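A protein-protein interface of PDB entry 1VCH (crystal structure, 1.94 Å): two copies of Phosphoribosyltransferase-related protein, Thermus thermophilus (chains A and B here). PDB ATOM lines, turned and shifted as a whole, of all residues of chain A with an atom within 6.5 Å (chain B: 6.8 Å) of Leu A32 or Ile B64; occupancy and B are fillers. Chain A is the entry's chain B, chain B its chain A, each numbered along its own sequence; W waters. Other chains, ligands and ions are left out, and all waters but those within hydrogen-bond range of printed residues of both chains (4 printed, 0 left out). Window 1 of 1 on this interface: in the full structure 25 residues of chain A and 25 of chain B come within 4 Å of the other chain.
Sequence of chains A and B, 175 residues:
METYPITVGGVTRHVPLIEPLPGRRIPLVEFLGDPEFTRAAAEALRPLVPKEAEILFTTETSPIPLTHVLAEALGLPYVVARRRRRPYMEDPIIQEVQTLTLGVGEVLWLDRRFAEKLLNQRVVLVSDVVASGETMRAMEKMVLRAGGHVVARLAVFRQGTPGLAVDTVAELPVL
Water W1 lies within hydrogen-bond range of the side-chain hydroxyl (OG1) of Thr A61 (2.5 Å), the side-chain hydroxyl (OG1) of Thr B61 (2.6 Å) and the side-chain carboxylate (OE1) of Glu B60 (2.8 Å). Water W3 bridges the side-chain hydroxyl of Thr A61 (2.7 Å) and the guanidinium group of Arg B82 (3.4 Å). Water W2 lies within hydrogen-bond range of the backbone carbonyl oxygen of Pro A35 (2.9 Å) and a ring nitrogen (NE2) of His B68 (2.9 Å). Water W4 bridges the backbone carbonyl oxygen (O) of Tyr B78 (2.9 Å) and the backbone carbonyl oxygen (O) of Gly A33 (3.0 Å).
Hydrophobic or aromatic side chains of chain A that line the printed part of chain B: Leu A32, Pro A35, Ile A64 and Pro A65. Printed residues of chain B that touch a printed residue of chain A: Leu B32, Glu B60, Thr B61, Ile B64, His B68, Tyr B78, Arg B82 and Phe B114. Among the printed residues, 15 pairs touch across the chains.
Leu A32 touches Ile B64. Leu A32 touches Tyr B78 (CA to OH, 3.9 Å). Phe B114 touches Leu A32 (CZ to O, 3.6 Å). Asp A34 touches Tyr B78 (N to CE1, 3.9 Å). Pro A35 touches His B68. CE1 of His B68 touches OG1 of Thr A38, 3.5 Å away. OG1 of Thr A61 touches OE1 of Glu B60 (3.8 Å). Thr A61 touches Ile B64 (CG2 to CD1, 3.6 Å). Leu B32 touches Ile A64. His B68 touches Pro A65.
Of chain B, only Ile B64 (3.7 Å), Tyr B78 (3.9 Å) and Phe B114 (3.6 Å) come within 4 Å of Leu A32. Ile B64 touches just these residues of chain A: Leu A32 and Thr A61. Printed residues of chain A within 4 Å of Glu B60: Thr A61. Printed residues of chain B within 4 Å of Pro A65: His B68 and Tyr B78. Of the printed residues of chain B, Ile A64 touches Leu B32 and Thr B61. Of the printed residues of chain B, Thr A61 touches Glu B60, Ile B64 and Arg B82. Ser B62 touches none of the printed residues of chain A. The nearest residue of chain B that does not touch Leu A32 is Val B80 (4.2 Å). The nearest printed residue of chain B that does not touch Thr A61 is Thr B61 (5.0 Å).
The backbone carbonyl oxygen (O) of Ala B81 lies within hydrogen-bond range of the backbone NH (N) of Glu B60, 3.0 Å away. OE1 of Glu B60 lies within salt-bridge range of NE of Arg B82, at 2.8 Å. ND1 of His B68 sits at hydrogen-bond distance from OH of Tyr B78, 2.5 Å away. N of Leu A32 sits at hydrogen-bond distance from OE1 of Glu A30 (3.0 Å). The backbone carbonyl oxygen of Phe A31 is in hydrogen-bond range of the side-chain hydroxyl of Thr A38, at 3.2 Å. O of Asp A34 sits at hydrogen-bond distance from OG1 of Thr A38.
Leu A32 touches Ile B64, and with the chains exchanged Ile A64 touches Leu B32. Thr A61 touches Ile B64, and with the chains exchanged Ile A64 touches Thr B61. 7 positions are printed for both chains. Of the 15 pairs that touch across the chains among the printed residues, 4 have their exchanged pair printed and touching as well.
OH of Tyr B78 lies close to N of Gly A33. NH2 of Arg B82 lies within hydrogen-bond range of OG1 of Thr A61, 3.3 Å away.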
ATOM      1  N   GLU A  30     -16.364  18.989 -18.063  1.00  0.00           N
ATOM      2  CA  GLU A  30     -17.261  18.871 -19.204  1.00  0.00           C
ATOM      3  C   GLU A  30     -17.540  20.242 -19.806  1.00  0.00           C
ATOM      4  O   GLU A  30     -18.145  21.103 -19.166  1.00  0.00           O
ATOM      5  CB  GLU A  30     -18.580  18.218 -18.773  1.00  0.00           C
ATOM      6  CG  GLU A  30     -19.624  18.053 -19.888  1.00  0.00           C
ATOM      7  CD  GLU A  30     -19.155  17.153 -21.025  1.00  0.00           C
ATOM      8  OE1 GLU A  30     -18.376  17.620 -21.889  1.00  0.00           O
ATOM      9  OE2 GLU A  30     -19.568  15.972 -21.055  1.00  0.00           O
ATOM     10  N   PHE A  31     -17.074  20.446 -21.029  1.00  0.00           N
ATOM     11  CA  PHE A  31     -17.312  21.706 -21.725  1.00  0.00           C
ATOM     12  C   PHE A  31     -18.612  21.627 -22.518  1.00  0.00           C
ATOM     13  O   PHE A  31     -19.229  22.657 -22.797  1.00  0.00           O
ATOM     14  CB  PHE A  31     -16.139  22.025 -22.656  1.00  0.00           C
ATOM     15  CG  PHE A  31     -14.893  22.422 -21.920  1.00  0.00           C
ATOM     16  CD1 PHE A  31     -14.883  23.568 -21.131  1.00  0.00           C
ATOM     17  CD2 PHE A  31     -13.749  21.636 -21.975  1.00  0.00           C
ATOM     18  CE1 PHE A  31     -13.752  23.931 -20.403  1.00  0.00           C
ATOM     19  CE2 PHE A  31     -12.615  21.991 -21.249  1.00  0.00           C
ATOM     20  CZ  PHE A  31     -12.619  23.144 -20.462  1.00  0.00           C
ATOM     21  N   LEU A  32     -19.031  20.415 -22.885  1.00  0.00           N
ATOM     22  CA  LEU A  32     -20.272  20.265 -23.647  1.00  0.00           C
ATOM     23  C   LEU A  32     -21.428  20.913 -22.908  1.00  0.00           C
ATOM     24  O   LEU A  32     -21.625  20.664 -21.716  1.00  0.00           O
ATOM     25  CB  LEU A  32     -20.641  18.798 -23.889  1.00  0.00           C
ATOM     26  CG  LEU A  32     -20.022  17.940 -24.995  1.00  0.00           C
ATOM     27  CD1 LEU A  32     -20.729  16.591 -24.961  1.00  0.00           C
ATOM     28  CD2 LEU A  32     -20.179  18.588 -26.379  1.00  0.00           C
ATOM     29  N   GLY A  33     -22.184  21.734 -23.633  1.00  0.00           N
ATOM     30  CA  GLY A  33     -23.338  22.414 -23.071  1.00  0.00           C
ATOM     31  C   GLY A  33     -23.048  23.683 -22.281  1.00  0.00           C
ATOM     32  O   GLY A  33     -23.981  24.351 -21.827  1.00  0.00           O
ATOM     33  N   ASP A  34     -21.774  24.051 -22.160  1.00  0.00           N
ATOM     34  CA  ASP A  34     -21.383  25.200 -21.349  1.00  0.00           C
ATOM     35  C   ASP A  34     -20.572  26.275 -22.088  1.00  0.00           C
ATOM     36  O   ASP A  34     -19.351  26.347 -21.960  1.00  0.00           O
ATOM     37  CB  ASP A  34     -20.578  24.686 -20.159  1.00  0.00           C
ATOM     38  CG  ASP A  34     -20.484  25.687 -19.036  1.00  0.00           C
ATOM     39  OD1 ASP A  34     -20.659  26.903 -19.272  1.00  0.00           O
ATOM     40  OD2 ASP A  34     -20.215  25.249 -17.909  1.00  0.00           O
ATOM     41  N   PRO A  35     -21.248  27.135 -22.865  1.00  0.00           N
ATOM     42  CA  PRO A  35     -20.555  28.193 -23.611  1.00  0.00           C
ATOM     43  C   PRO A  35     -19.616  29.086 -22.801  1.00  0.00           C
ATOM     44  O   PRO A  35     -18.499  29.348 -23.223  1.00  0.00           O
ATOM     45  CB  PRO A  35     -21.703  28.977 -24.237  1.00  0.00           C
ATOM     46  CG  PRO A  35     -22.718  27.902 -24.507  1.00  0.00           C
ATOM     47  CD  PRO A  35     -22.678  27.086 -23.218  1.00  0.00           C
ATOM     48  N   THR A  38     -16.554  27.123 -21.686  1.00  0.00           N
ATOM     49  CA  THR A  38     -15.786  26.797 -22.886  1.00  0.00           C
ATOM     50  C   THR A  38     -15.011  28.027 -23.380  1.00  0.00           C
ATOM     51  O   THR A  38     -13.841  27.934 -23.764  1.00  0.00           O
ATOM     52  CB  THR A  38     -16.720  26.275 -24.011  1.00  0.00           C
ATOM     53  OG1 THR A  38     -17.324  25.045 -23.592  1.00  0.00           O
ATOM     54  CG2 THR A  38     -15.931  26.006 -25.299  1.00  0.00           C
ATOM     55  N   THR A  61     -15.412  13.565 -27.588  1.00  0.00           N
ATOM     56  CA  THR A  61     -16.494  14.462 -27.968  1.00  0.00           C
ATOM     57  C   THR A  61     -16.418  15.783 -27.214  1.00  0.00           C
ATOM     58  O   THR A  61     -16.575  16.855 -27.796  1.00  0.00           O
ATOM     59  CB  THR A  61     -17.861  13.805 -27.660  1.00  0.00           C
ATOM     60  OG1 THR A  61     -17.958  12.570 -28.381  1.00  0.00           O
ATOM     61  CG2 THR A  61     -19.018  14.734 -28.058  1.00  0.00           C
ATOM     62  N   SER A  62     -16.177  15.701 -25.911  1.00  0.00           N
ATOM     63  CA  SER A  62     -16.101  16.887 -25.071  1.00  0.00           C
ATOM     64  C   SER A  62     -15.174  17.997 -25.562  1.00  0.00           C
ATOM     65  O   SER A  62     -15.485  19.177 -25.401  1.00  0.00           O
ATOM     66  CB  SER A  62     -15.714  16.490 -23.639  1.00  0.00           C
ATOM     67  OG  SER A  62     -16.818  15.889 -22.979  1.00  0.00           O
ATOM     68  N   PRO A  63     -14.022  17.639 -26.152  1.00  0.00           N
ATOM     69  CA  PRO A  63     -13.084  18.655 -26.643  1.00  0.00           C
ATOM     70  C   PRO A  63     -13.565  19.428 -27.861  1.00  0.00           C
ATOM     71  O   PRO A  63     -12.988  20.459 -28.208  1.00  0.00           O
ATOM     72  CB  PRO A  63     -11.831  17.844 -26.974  1.00  0.00           C
ATOM     73  CG  PRO A  63     -11.922  16.663 -26.057  1.00  0.00           C
ATOM     74  CD  PRO A  63     -13.385  16.309 -26.147  1.00  0.00           C
ATOM     75  N   ILE A  64     -14.619  18.934 -28.505  1.00  0.00           N
ATOM     76  CA  ILE A  64     -15.111  19.567 -29.721  1.00  0.00           C
ATOM     77  C   ILE A  64     -15.476  21.045 -29.577  1.00  0.00           C
ATOM     78  O   ILE A  64     -14.960  21.876 -30.317  1.00  0.00           O
ATOM     79  CB  ILE A  64     -16.293  18.768 -30.321  1.00  0.00           C
ATOM     80  CG1 ILE A  64     -15.791  17.392 -30.785  1.00  0.00           C
ATOM     81  CG2 ILE A  64     -16.913  19.538 -31.505  1.00  0.00           C
ATOM     82  CD1 ILE A  64     -16.866  16.475 -31.365  1.00  0.00           C
ATOM     83  N   PRO A  65     -16.362  21.393 -28.630  1.00  0.00           N
ATOM     84  CA  PRO A  65     -16.707  22.815 -28.494  1.00  0.00           C
ATOM     85  C   PRO A  65     -15.490  23.680 -28.137  1.00  0.00           C
ATOM     86  O   PRO A  65     -15.351  24.802 -28.617  1.00  0.00           O
ATOM     87  CB  PRO A  65     -17.795  22.811 -27.415  1.00  0.00           C
ATOM     88  CG  PRO A  65     -17.531  21.533 -26.639  1.00  0.00           C
ATOM     89  CD  PRO A  65     -17.164  20.558 -27.716  1.00  0.00           C
ATOM     90  N   LEU B  32     -18.516  19.937 -38.530  1.00  0.00           N
ATOM     91  CA  LEU B  32     -17.321  19.690 -37.726  1.00  0.00           C
ATOM     92  C   LEU B  32     -16.065  20.119 -38.478  1.00  0.00           C
ATOM     93  O   LEU B  32     -15.854  19.710 -39.623  1.00  0.00           O
ATOM     94  CB  LEU B  32     -17.182  18.207 -37.386  1.00  0.00           C
ATOM     95  CG  LEU B  32     -18.091  17.513 -36.375  1.00  0.00           C
ATOM     96  CD1 LEU B  32     -17.772  16.019 -36.402  1.00  0.00           C
ATOM     97  CD2 LEU B  32     -17.871  18.084 -34.981  1.00  0.00           C
ATOM     98  N   THR B  38     -20.097  26.894 -40.070  1.00  0.00           N
ATOM     99  CA  THR B  38     -20.931  26.705 -38.886  1.00  0.00           C
ATOM    100  C   THR B  38     -21.516  28.040 -38.431  1.00  0.00           C
ATOM    101  O   THR B  38     -22.673  28.116 -38.028  1.00  0.00           O
ATOM    102  CB  THR B  38     -20.127  26.099 -37.712  1.00  0.00           C
ATOM    103  OG1 THR B  38     -19.649  24.798 -38.086  1.00  0.00           O
ATOM    104  CG2 THR B  38     -21.024  25.970 -36.469  1.00  0.00           C
ATOM    105  N   THR B  58     -29.499  19.142 -28.580  1.00  0.00           N
ATOM    106  CA  THR B  58     -29.039  18.552 -29.827  1.00  0.00           C
ATOM    107  C   THR B  58     -28.477  17.160 -29.537  1.00  0.00           C
ATOM    108  O   THR B  58     -28.387  16.747 -28.370  1.00  0.00           O
ATOM    109  CB  THR B  58     -27.944  19.433 -30.499  1.00  0.00           C
ATOM    110  OG1 THR B  58     -27.707  18.965 -31.832  1.00  0.00           O
ATOM    111  CG2 THR B  58     -26.628  19.358 -29.713  1.00  0.00           C
ATOM    112  N   THR B  59     -28.127  16.437 -30.598  1.00  0.00           N
ATOM    113  CA  THR B  59     -27.549  15.100 -30.483  1.00  0.00           C
ATOM    114  C   THR B  59     -26.164  15.138 -31.130  1.00  0.00           C
ATOM    115  O   THR B  59     -25.909  15.937 -32.040  1.00  0.00           O
ATOM    116  CB  THR B  59     -28.424  14.024 -31.198  1.00  0.00           C
ATOM    117  OG1 THR B  59     -29.732  13.996 -30.616  1.00  0.00           O
ATOM    118  CG2 THR B  59     -27.811  12.637 -31.041  1.00  0.00           C
ATOM    119  N   GLU B  60     -25.261  14.294 -30.648  1.00  0.00           N
ATOM    120  CA  GLU B  60     -23.912  14.241 -31.199  1.00  0.00           C
ATOM    121  C   GLU B  60     -23.994  13.635 -32.615  1.00  0.00           C
ATOM    122  O   GLU B  60     -24.951  12.922 -32.925  1.00  0.00           O
ATOM    123  CB  GLU B  60     -23.028  13.377 -30.291  1.00  0.00           C
ATOM    124  CG  GLU B  60     -23.436  11.904 -30.266  1.00  0.00           C
ATOM    125  CD  GLU B  60     -22.556  11.070 -29.349  1.00  0.00           C
ATOM    126  OE1 GLU B  60     -21.581  11.615 -28.794  1.00  0.00           O
ATOM    127  OE2 GLU B  60     -22.833   9.865 -29.187  1.00  0.00           O
ATOM    128  N   THR B  61     -22.999  13.882 -33.466  1.00  0.00           N
ATOM    129  CA  THR B  61     -21.820  14.678 -33.150  1.00  0.00           C
ATOM    130  C   THR B  61     -21.741  15.997 -33.946  1.00  0.00           C
ATOM    131  O   THR B  61     -21.509  17.067 -33.384  1.00  0.00           O
ATOM    132  CB  THR B  61     -20.554  13.858 -33.442  1.00  0.00           C
ATOM    133  OG1 THR B  61     -20.611  12.626 -32.710  1.00  0.00           O
ATOM    134  CG2 THR B  61     -19.302  14.633 -33.045  1.00  0.00           C
ATOM    135  N   SER B  62     -21.927  15.918 -35.258  1.00  0.00           N
ATOM    136  CA  SER B  62     -21.853  17.109 -36.101  1.00  0.00           C
ATOM    137  C   SER B  62     -22.669  18.333 -35.649  1.00  0.00           C
ATOM    138  O   SER B  62     -22.204  19.464 -35.779  1.00  0.00           O
ATOM    139  CB  SER B  62     -22.220  16.739 -37.541  1.00  0.00           C
ATOM    140  OG  SER B  62     -21.291  15.796 -38.051  1.00  0.00           O
ATOM    141  N   PRO B  63     -23.885  18.133 -35.106  1.00  0.00           N
ATOM    142  CA  PRO B  63     -24.697  19.275 -34.660  1.00  0.00           C
ATOM    143  C   PRO B  63     -24.168  20.021 -33.426  1.00  0.00           C
ATOM    144  O   PRO B  63     -24.653  21.101 -33.098  1.00  0.00           O
ATOM    145  CB  PRO B  63     -26.066  18.643 -34.376  1.00  0.00           C
ATOM    146  CG  PRO B  63     -26.074  17.401 -35.213  1.00  0.00           C
ATOM    147  CD  PRO B  63     -24.670  16.888 -35.043  1.00  0.00           C
ATOM    148  N   ILE B  64     -23.190  19.442 -32.733  1.00  0.00           N
ATOM    149  CA  ILE B  64     -22.651  20.071 -31.531  1.00  0.00           C
ATOM    150  C   ILE B  64     -22.068  21.476 -31.730  1.00  0.00           C
ATOM    151  O   ILE B  64     -22.451  22.406 -31.029  1.00  0.00           O
ATOM    152  CB  ILE B  64     -21.592  19.163 -30.857  1.00  0.00           C
ATOM    153  CG1 ILE B  64     -22.290  17.921 -30.280  1.00  0.00           C
ATOM    154  CG2 ILE B  64     -20.861  19.934 -29.744  1.00  0.00           C
ATOM    155  CD1 ILE B  64     -21.342  16.855 -29.753  1.00  0.00           C
ATOM    156  N   PRO B  65     -21.123  21.644 -32.671  1.00  0.00           N
ATOM    157  CA  PRO B  65     -20.575  22.991 -32.855  1.00  0.00           C
ATOM    158  C   PRO B  65     -21.661  23.973 -33.307  1.00  0.00           C
ATOM    159  O   PRO B  65     -21.687  25.126 -32.880  1.00  0.00           O
ATOM    160  CB  PRO B  65     -19.462  22.782 -33.891  1.00  0.00           C
ATOM    161  CG  PRO B  65     -19.894  21.564 -34.635  1.00  0.00           C
ATOM    162  CD  PRO B  65     -20.461  20.675 -33.558  1.00  0.00           C
ATOM    163  N   LEU B  66     -22.564  23.496 -34.157  1.00  0.00           N
ATOM    164  CA  LEU B  66     -23.666  24.319 -34.636  1.00  0.00           C
ATOM    165  C   LEU B  66     -24.475  24.822 -33.432  1.00  0.00           C
ATOM    166  O   LEU B  66     -24.701  26.025 -33.263  1.00  0.00           O
ATOM    167  CB  LEU B  66     -24.558  23.486 -35.564  1.00  0.00           C
ATOM    168  CG  LEU B  66     -25.935  24.053 -35.927  1.00  0.00           C
ATOM    169  CD1 LEU B  66     -25.775  25.351 -36.718  1.00  0.00           C
ATOM    170  CD2 LEU B  66     -26.694  23.035 -36.739  1.00  0.00           C
ATOM    171  N   THR B  67     -24.889  23.882 -32.587  1.00  0.00           N
ATOM    172  CA  THR B  67     -25.686  24.186 -31.404  1.00  0.00           C
ATOM    173  C   THR B  67     -24.935  25.034 -30.386  1.00  0.00           C
ATOM    174  O   THR B  67     -25.512  25.899 -29.725  1.00  0.00           O
ATOM    175  CB  THR B  67     -26.160  22.866 -30.732  1.00  0.00           C
ATOM    176  OG1 THR B  67     -26.967  22.127 -31.653  1.00  0.00           O
ATOM    177  CG2 THR B  67     -26.953  23.144 -29.479  1.00  0.00           C
ATOM    178  N   HIS B  68     -23.641  24.778 -30.247  1.00  0.00           N
ATOM    179  CA  HIS B  68     -22.824  25.521 -29.297  1.00  0.00           C
ATOM    180  C   HIS B  68     -22.741  26.991 -29.708  1.00  0.00           C
ATOM    181  O   HIS B  68     -22.982  27.898 -28.906  1.00  0.00           O
ATOM    182  CB  HIS B  68     -21.399  24.935 -29.254  1.00  0.00           C
ATOM    183  CG  HIS B  68     -20.553  25.511 -28.162  1.00  0.00           C
ATOM    184  ND1 HIS B  68     -20.376  24.882 -26.950  1.00  0.00           N
ATOM    185  CD2 HIS B  68     -19.875  26.679 -28.083  1.00  0.00           C
ATOM    186  CE1 HIS B  68     -19.625  25.639 -26.171  1.00  0.00           C
ATOM    187  NE2 HIS B  68     -19.308  26.736 -26.835  1.00  0.00           N
ATOM    188  N   VAL B  69     -22.390  27.211 -30.970  1.00  0.00           N
ATOM    189  CA  VAL B  69     -22.261  28.561 -31.511  1.00  0.00           C
ATOM    190  C   VAL B  69     -23.592  29.318 -31.379  1.00  0.00           C
ATOM    191  O   VAL B  69     -23.626  30.467 -30.930  1.00  0.00           O
ATOM    192  CB  VAL B  69     -21.806  28.493 -32.992  1.00  0.00           C
ATOM    193  CG1 VAL B  69     -21.830  29.871 -33.632  1.00  0.00           C
ATOM    194  CG2 VAL B  69     -20.393  27.918 -33.047  1.00  0.00           C
ATOM    195  N   LEU B  70     -24.684  28.658 -31.747  1.00  0.00           N
ATOM    196  CA  LEU B  70     -26.006  29.274 -31.642  1.00  0.00           C
ATOM    197  C   LEU B  70     -26.336  29.613 -30.186  1.00  0.00           C
ATOM    198  O   LEU B  70     -26.813  30.711 -29.873  1.00  0.00           O
ATOM    199  CB  LEU B  70     -27.076  28.330 -32.191  1.00  0.00           C
ATOM    200  CG  LEU B  70     -28.500  28.864 -32.009  1.00  0.00           C
ATOM    201  CD1 LEU B  70     -28.634  30.201 -32.799  1.00  0.00           C
ATOM    202  CD2 LEU B  70     -29.505  27.842 -32.504  1.00  0.00           C
ATOM    203  N   TYR B  78     -27.081  24.579 -23.295  1.00  0.00           N
ATOM    204  CA  TYR B  78     -27.618  23.553 -24.169  1.00  0.00           C
ATOM    205  C   TYR B  78     -27.218  22.196 -23.613  1.00  0.00           C
ATOM    206  O   TYR B  78     -26.376  22.121 -22.728  1.00  0.00           O
ATOM    207  CB  TYR B  78     -27.120  23.709 -25.617  1.00  0.00           C
ATOM    208  CG  TYR B  78     -25.641  23.458 -25.851  1.00  0.00           C
ATOM    209  CD1 TYR B  78     -24.690  24.443 -25.573  1.00  0.00           C
ATOM    210  CD2 TYR B  78     -25.196  22.234 -26.353  1.00  0.00           C
ATOM    211  CE1 TYR B  78     -23.316  24.212 -25.787  1.00  0.00           C
ATOM    212  CE2 TYR B  78     -23.826  21.989 -26.570  1.00  0.00           C
ATOM    213  CZ  TYR B  78     -22.897  22.981 -26.281  1.00  0.00           C
ATOM    214  OH  TYR B  78     -21.543  22.733 -26.445  1.00  0.00           O
ATOM    215  N   VAL B  79     -27.855  21.142 -24.095  1.00  0.00           N
ATOM    216  CA  VAL B  79     -27.504  19.798 -23.662  1.00  0.00           C
ATOM    217  C   VAL B  79     -27.329  18.942 -24.901  1.00  0.00           C
ATOM    218  O   VAL B  79     -27.830  19.275 -25.972  1.00  0.00           O
ATOM    219  CB  VAL B  79     -28.575  19.180 -22.735  1.00  0.00           C
ATOM    220  CG1 VAL B  79     -28.680  20.014 -21.458  1.00  0.00           C
ATOM    221  CG2 VAL B  79     -29.912  19.092 -23.453  1.00  0.00           C
ATOM    222  N   VAL B  80     -26.623  17.831 -24.743  1.00  0.00           N
ATOM    223  CA  VAL B  80     -26.338  16.940 -25.848  1.00  0.00           C
ATOM    224  C   VAL B  80     -26.665  15.492 -25.530  1.00  0.00           C
ATOM    225  O   VAL B  80     -26.193  14.953 -24.528  1.00  0.00           O
ATOM    226  CB  VAL B  80     -24.836  17.016 -26.207  1.00  0.00           C
ATOM    227  CG1 VAL B  80     -24.540  16.147 -27.409  1.00  0.00           C
ATOM    228  CG2 VAL B  80     -24.422  18.474 -26.431  1.00  0.00           C
ATOM    229  N   ALA B  81     -27.474  14.866 -26.379  1.00  0.00           N
ATOM    230  CA  ALA B  81     -27.800  13.456 -26.206  1.00  0.00           C
ATOM    231  C   ALA B  81     -26.710  12.704 -26.966  1.00  0.00           C
ATOM    232  O   ALA B  81     -26.223  13.186 -28.003  1.00  0.00           O
ATOM    233  CB  ALA B  81     -29.178  13.137 -26.803  1.00  0.00           C
ATOM    234  N   ARG B  82     -26.317  11.542 -26.449  1.00  0.00           N
ATOM    235  CA  ARG B  82     -25.281  10.731 -27.080  1.00  0.00           C
ATOM    236  C   ARG B  82     -25.975   9.569 -27.789  1.00  0.00           C
ATOM    237  O   ARG B  82     -27.142   9.278 -27.517  1.00  0.00           O
ATOM    238  CB  ARG B  82     -24.300  10.192 -26.018  1.00  0.00           C
ATOM    239  CG  ARG B  82     -23.893  11.219 -24.963  1.00  0.00           C
ATOM    240  CD  ARG B  82     -23.165  12.397 -25.579  1.00  0.00           C
ATOM    241  NE  ARG B  82     -21.813  12.034 -25.988  1.00  0.00           N
ATOM    242  CZ  ARG B  82     -20.752  12.061 -25.185  1.00  0.00           C
ATOM    243  NH1 ARG B  82     -20.871  12.447 -23.919  1.00  0.00           N
ATOM    244  NH2 ARG B  82     -19.568  11.692 -25.651  1.00  0.00           N
ATOM    245  N   PHE B 114     -27.587  16.515 -17.488  1.00  0.00           N
ATOM    246  CA  PHE B 114     -28.153  17.330 -18.562  1.00  0.00           C
ATOM    247  C   PHE B 114     -29.679  17.382 -18.427  1.00  0.00           C
ATOM    248  O   PHE B 114     -30.307  18.424 -18.638  1.00  0.00           O
ATOM    249  CB  PHE B 114     -27.812  16.739 -19.933  1.00  0.00           C
ATOM    250  CG  PHE B 114     -26.467  17.157 -20.474  1.00  0.00           C
ATOM    251  CD1 PHE B 114     -25.909  18.388 -20.135  1.00  0.00           C
ATOM    252  CD2 PHE B 114     -25.790  16.343 -21.378  1.00  0.00           C
ATOM    253  CE1 PHE B 114     -24.704  18.801 -20.694  1.00  0.00           C
ATOM    254  CE2 PHE B 114     -24.581  16.750 -21.940  1.00  0.00           C
ATOM    255  CZ  PHE B 114     -24.040  17.977 -21.599  1.00  0.00           C
HETATM  256  O   HOH W   1     -19.429  12.455 -30.423  1.00  0.00           O
HETATM  257  O   HOH W   2     -17.861  29.095 -26.004  1.00  0.00           O
HETATM  258  O   HOH W   3     -16.756  10.536 -27.083  1.00  0.00           O
HETATM  259  O   HOH W   4     -25.704  22.730 -19.999  1.00  0.00           O
